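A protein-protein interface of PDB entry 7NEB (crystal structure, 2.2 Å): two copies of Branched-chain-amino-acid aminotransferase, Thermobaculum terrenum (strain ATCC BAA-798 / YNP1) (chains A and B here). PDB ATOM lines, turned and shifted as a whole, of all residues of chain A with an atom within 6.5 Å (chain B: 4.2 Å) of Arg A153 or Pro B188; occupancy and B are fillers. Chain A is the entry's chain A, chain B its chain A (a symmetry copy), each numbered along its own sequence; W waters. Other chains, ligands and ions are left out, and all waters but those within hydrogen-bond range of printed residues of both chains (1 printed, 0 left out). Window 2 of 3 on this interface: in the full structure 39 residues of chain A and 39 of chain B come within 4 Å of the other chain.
O of Arg A153 lies within hydrogen-bond range of N of Thr B148 (3.0 Å). The guanidinium group of Arg A153 sits at hydrogen-bond distance from the backbone carbonyl oxygen of Pro B188.
Among the printed residues, merely in contact across the chains: Glu A152 with Trp B147 (3.3 Å), Val A154 with Arg B149 (3.5 Å), Val A154 with Thr B148 (3.6 Å), Pro A156 with Trp B147 (3.9 Å) and Arg A153 with Trp B147 (3.9 Å).
Printed residues of chain B within 4 Å of Glu A152: Trp B147. Arg A153 touches three residues of chain B. Of the printed residues of chain B, Val A154 touches Thr B148 and Arg B149. Of the printed residues of chain B, Pro A156 touches Trp B147 (3.9 Å). The nearest printed residue of chain A that does not touch Arg B149 is Arg A153 (5.4 Å).
Of the 8 printed residues of chain B, 4 touch a printed residue of chain A. Printed residues of chain A that touch a printed residue of chain B: Glu A152, Arg A153, Val A154 and Pro A156. Among the printed residues, 7 pairs touch across the chains.
Positions printed for both chains: 151 and 189. Of the 7 pairs that touch across the chains among the printed residues, none has its exchanged pair printed and touching as well.
Water W1 bridges the side-chain hydroxyl (OG1) of Thr B148 and the backbone carbonyl oxygen (O) of Arg A153.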
ATOM      1  N   ASN A 151      -9.811   3.869 -27.200  1.00  0.00           N
ATOM      2  CA  ASN A 151     -10.868   3.518 -28.198  1.00  0.00           C
ATOM      3  C   ASN A 151     -12.007   2.747 -27.505  1.00  0.00           C
ATOM      4  O   ASN A 151     -11.819   2.327 -26.286  1.00  0.00           O
ATOM      5  CB  ASN A 151     -10.283   2.731 -29.384  1.00  0.00           C
ATOM      6  CG  ASN A 151      -9.750   1.378 -28.956  1.00  0.00           C
ATOM      7  OD1 ASN A 151      -9.528   1.116 -27.753  1.00  0.00           O
ATOM      8  ND2 ASN A 151      -9.548   0.511 -29.935  1.00  0.00           N
ATOM      9  N   GLU A 152     -13.097   2.512 -28.262  1.00  0.00           N
ATOM     10  CA  GLU A 152     -14.315   1.770 -27.785  1.00  0.00           C
ATOM     11  C   GLU A 152     -13.946   0.363 -27.246  1.00  0.00           C
ATOM     12  O   GLU A 152     -14.542  -0.094 -26.244  1.00  0.00           O
ATOM     13  CB  GLU A 152     -15.373   1.710 -28.902  1.00  0.00           C
ATOM     14  CG  GLU A 152     -16.077   3.055 -29.137  1.00  0.00           C
ATOM     15  CD  GLU A 152     -17.311   3.398 -28.291  1.00  0.00           C
ATOM     16  OE1 GLU A 152     -18.153   2.471 -28.064  1.00  0.00           O
ATOM     17  OE2 GLU A 152     -17.458   4.622 -27.896  1.00  0.00           O
ATOM     18  N   ARG A 153     -12.946  -0.285 -27.837  1.00  0.00           N
ATOM     19  CA  ARG A 153     -12.474  -1.623 -27.402  1.00  0.00           C
ATOM     20  C   ARG A 153     -12.108  -1.625 -25.893  1.00  0.00           C
ATOM     21  O   ARG A 153     -12.407  -2.649 -25.210  1.00  0.00           O
ATOM     22  CB  ARG A 153     -11.297  -1.995 -28.304  1.00  0.00           C
ATOM     23  CG  ARG A 153     -11.684  -2.178 -29.778  1.00  0.00           C
ATOM     24  CD  ARG A 153     -10.699  -3.054 -30.531  1.00  0.00           C
ATOM     25  NE  ARG A 153     -10.673  -4.381 -29.910  1.00  0.00           N
ATOM     26  CZ  ARG A 153      -9.641  -5.234 -29.896  1.00  0.00           C
ATOM     27  NH1 ARG A 153      -8.483  -4.968 -30.510  1.00  0.00           N
ATOM     28  NH2 ARG A 153      -9.786  -6.386 -29.261  1.00  0.00           N
ATOM     29  N   VAL A 154     -11.510  -0.533 -25.376  1.00  0.00           N
ATOM     30  CA  VAL A 154     -10.871  -0.461 -24.015  1.00  0.00           C
ATOM     31  C   VAL A 154     -11.577   0.589 -23.121  1.00  0.00           C
ATOM     32  O   VAL A 154     -11.698   0.322 -21.924  1.00  0.00           O
ATOM     33  CB  VAL A 154      -9.327  -0.259 -24.100  1.00  0.00           C
ATOM     34  CG1 VAL A 154      -8.651  -1.359 -24.949  1.00  0.00           C
ATOM     35  CG2 VAL A 154      -8.886   1.138 -24.579  1.00  0.00           C
ATOM     36  N   LEU A 155     -11.955   1.762 -23.649  1.00  0.00           N
ATOM     37  CA  LEU A 155     -12.382   2.940 -22.837  1.00  0.00           C
ATOM     38  C   LEU A 155     -13.195   3.887 -23.746  1.00  0.00           C
ATOM     39  O   LEU A 155     -12.644   4.839 -24.304  1.00  0.00           O
ATOM     40  CB  LEU A 155     -11.123   3.602 -22.225  1.00  0.00           C
ATOM     41  CG  LEU A 155     -10.580   3.190 -20.827  1.00  0.00           C
ATOM     42  CD1 LEU A 155      -9.802   4.355 -20.172  1.00  0.00           C
ATOM     43  CD2 LEU A 155     -11.646   2.740 -19.840  1.00  0.00           C
ATOM     44  N   PRO A 156     -14.527   3.670 -23.964  1.00  0.00           N
ATOM     45  CA  PRO A 156     -15.307   4.507 -24.889  1.00  0.00           C
ATOM     46  C   PRO A 156     -15.025   5.990 -24.713  1.00  0.00           C
ATOM     47  O   PRO A 156     -15.362   6.566 -23.687  1.00  0.00           O
ATOM     48  CB  PRO A 156     -16.755   4.127 -24.579  1.00  0.00           C
ATOM     49  CG  PRO A 156     -16.563   2.651 -24.324  1.00  0.00           C
ATOM     50  CD  PRO A 156     -15.371   2.614 -23.382  1.00  0.00           C
ATOM     51  N   PRO A 157     -14.405   6.638 -25.717  1.00  0.00           N
ATOM     52  CA  PRO A 157     -14.226   8.086 -25.695  1.00  0.00           C
ATOM     53  C   PRO A 157     -15.567   8.822 -25.494  1.00  0.00           C
ATOM     54  O   PRO A 157     -15.578  10.004 -25.015  1.00  0.00           O
ATOM     55  CB  PRO A 157     -13.687   8.389 -27.121  1.00  0.00           C
ATOM     56  CG  PRO A 157     -13.028   7.118 -27.575  1.00  0.00           C
ATOM     57  CD  PRO A 157     -13.857   6.020 -26.944  1.00  0.00           C
ATOM     58  N   GLU A 189      -5.536   3.111 -35.123  1.00  0.00           N
ATOM     59  CA  GLU A 189      -5.339   2.910 -36.589  1.00  0.00           C
ATOM     60  C   GLU A 189      -4.442   4.026 -37.202  1.00  0.00           C
ATOM     61  O   GLU A 189      -4.310   3.992 -38.447  1.00  0.00           O
ATOM     62  CB  GLU A 189      -6.721   2.751 -37.267  1.00  0.00           C
ATOM     63  CG  GLU A 189      -7.474   1.443 -36.932  1.00  0.00           C
ATOM     64  CD  GLU A 189      -7.932   1.215 -35.478  1.00  0.00           C
ATOM     65  OE1 GLU A 189      -8.506   2.182 -34.845  1.00  0.00           O
ATOM     66  OE2 GLU A 189      -7.668   0.081 -34.944  1.00  0.00           O
ATOM     67  N   TRP B 147     -15.129  -6.753 -23.370  1.00  0.00           N
ATOM     68  CA  TRP B 147     -14.222  -5.583 -23.263  1.00  0.00           C
ATOM     69  C   TRP B 147     -12.734  -6.019 -23.203  1.00  0.00           C
ATOM     70  O   TRP B 147     -12.379  -6.898 -22.407  1.00  0.00           O
ATOM     71  CB  TRP B 147     -14.606  -4.731 -22.058  1.00  0.00           C
ATOM     72  CG  TRP B 147     -16.026  -4.268 -22.086  1.00  0.00           C
ATOM     73  CD1 TRP B 147     -17.071  -4.853 -21.433  1.00  0.00           C
ATOM     74  CD2 TRP B 147     -16.562  -3.135 -22.794  1.00  0.00           C
ATOM     75  NE1 TRP B 147     -18.239  -4.216 -21.752  1.00  0.00           N
ATOM     76  CE2 TRP B 147     -17.966  -3.143 -22.561  1.00  0.00           C
ATOM     77  CE3 TRP B 147     -16.016  -2.147 -23.641  1.00  0.00           C
ATOM     78  CZ2 TRP B 147     -18.813  -2.153 -23.067  1.00  0.00           C
ATOM     79  CZ3 TRP B 147     -16.867  -1.214 -24.203  1.00  0.00           C
ATOM     80  CH2 TRP B 147     -18.246  -1.217 -23.913  1.00  0.00           C
ATOM     81  N   THR B 148     -11.896  -5.314 -23.960  1.00  0.00           N
ATOM     82  CA  THR B 148     -10.454  -5.577 -24.204  1.00  0.00           C
ATOM     83  C   THR B 148      -9.604  -4.887 -23.131  1.00  0.00           C
ATOM     84  O   THR B 148      -9.983  -3.781 -22.690  1.00  0.00           O
ATOM     85  CB  THR B 148     -10.076  -5.080 -25.603  1.00  0.00           C
ATOM     86  OG1 THR B 148     -11.020  -5.526 -26.596  1.00  0.00           O
ATOM     87  CG2 THR B 148      -8.659  -5.477 -25.977  1.00  0.00           C
ATOM     88  N   ARG B 149      -8.503  -5.509 -22.706  1.00  0.00           N
ATOM     89  CA  ARG B 149      -7.618  -4.896 -21.684  1.00  0.00           C
ATOM     90  C   ARG B 149      -6.920  -3.694 -22.353  1.00  0.00           C
ATOM     91  O   ARG B 149      -6.592  -3.795 -23.577  1.00  0.00           O
ATOM     92  CB  ARG B 149      -6.603  -5.918 -21.136  1.00  0.00           C
ATOM     93  CG  ARG B 149      -5.742  -5.517 -19.939  1.00  0.00           C
ATOM     94  CD  ARG B 149      -6.571  -4.861 -18.862  1.00  0.00           C
ATOM     95  NE  ARG B 149      -5.927  -4.615 -17.576  1.00  0.00           N
ATOM     96  CZ  ARG B 149      -6.466  -3.933 -16.544  1.00  0.00           C
ATOM     97  NH1 ARG B 149      -7.695  -3.405 -16.609  1.00  0.00           N
ATOM     98  NH2 ARG B 149      -5.765  -3.796 -15.423  1.00  0.00           N
ATOM     99  N   ASN B 151      -3.671  -1.393 -22.989  1.00  0.00           N
ATOM    100  CA  ASN B 151      -2.291  -1.794 -23.402  1.00  0.00           C
ATOM    101  C   ASN B 151      -1.339  -0.590 -23.282  1.00  0.00           C
ATOM    102  O   ASN B 151      -1.853   0.589 -23.076  1.00  0.00           O
ATOM    103  CB  ASN B 151      -2.280  -2.394 -24.819  1.00  0.00           C
ATOM    104  CG  ASN B 151      -2.670  -1.372 -25.868  1.00  0.00           C
ATOM    105  OD1 ASN B 151      -3.239  -0.302 -25.556  1.00  0.00           O
ATOM    106  ND2 ASN B 151      -2.362  -1.691 -27.115  1.00  0.00           N
ATOM    107  N   ASN B 187      -6.406  -9.396 -24.416  1.00  0.00           N
ATOM    108  CA  ASN B 187      -5.597  -8.212 -24.767  1.00  0.00           C
ATOM    109  C   ASN B 187      -6.074  -7.805 -26.152  1.00  0.00           C
ATOM    110  O   ASN B 187      -6.799  -8.603 -26.775  1.00  0.00           O
ATOM    111  CB  ASN B 187      -4.088  -8.445 -24.595  1.00  0.00           C
ATOM    112  CG  ASN B 187      -3.449  -9.402 -25.587  1.00  0.00           C
ATOM    113  OD1 ASN B 187      -4.047  -9.821 -26.602  1.00  0.00           O
ATOM    114  ND2 ASN B 187      -2.217  -9.786 -25.258  1.00  0.00           N
ATOM    115  N   PRO B 188      -5.636  -6.601 -26.658  1.00  0.00           N
ATOM    116  CA  PRO B 188      -6.000  -6.147 -28.012  1.00  0.00           C
ATOM    117  C   PRO B 188      -5.807  -7.219 -29.111  1.00  0.00           C
ATOM    118  O   PRO B 188      -6.685  -7.332 -29.968  1.00  0.00           O
ATOM    119  CB  PRO B 188      -5.145  -4.859 -28.198  1.00  0.00           C
ATOM    120  CG  PRO B 188      -4.903  -4.332 -26.785  1.00  0.00           C
ATOM    121  CD  PRO B 188      -4.747  -5.608 -25.972  1.00  0.00           C
ATOM    122  N   GLU B 189      -4.755  -8.056 -28.994  1.00  0.00           N
ATOM    123  CA  GLU B 189      -4.397  -9.145 -29.950  1.00  0.00           C
ATOM    124  C   GLU B 189      -5.217 -10.440 -29.672  1.00  0.00           C
ATOM    125  O   GLU B 189      -4.905 -11.437 -30.361  1.00  0.00           O
ATOM    126  CB  GLU B 189      -2.862  -9.342 -29.939  1.00  0.00           C
ATOM    127  CG  GLU B 189      -2.043  -8.185 -30.556  1.00  0.00           C
ATOM    128  CD  GLU B 189      -2.079  -6.811 -29.860  1.00  0.00           C
ATOM    129  OE1 GLU B 189      -1.944  -6.758 -28.577  1.00  0.00           O
ATOM    130  OE2 GLU B 189      -2.297  -5.781 -30.589  1.00  0.00           O
ATOM    131  N   GLY B 190      -6.196 -10.476 -28.737  1.00  0.00           N
ATOM    132  CA  GLY B 190      -6.995 -11.698 -28.444  1.00  0.00           C
ATOM    133  C   GLY B 190      -6.351 -12.686 -27.458  1.00  0.00           C
ATOM    134  O   GLY B 190      -6.913 -13.787 -27.243  1.00  0.00           O
HETATM  135  O   HOH W   1     -13.918  -4.996 -26.943  1.00  0.00           O
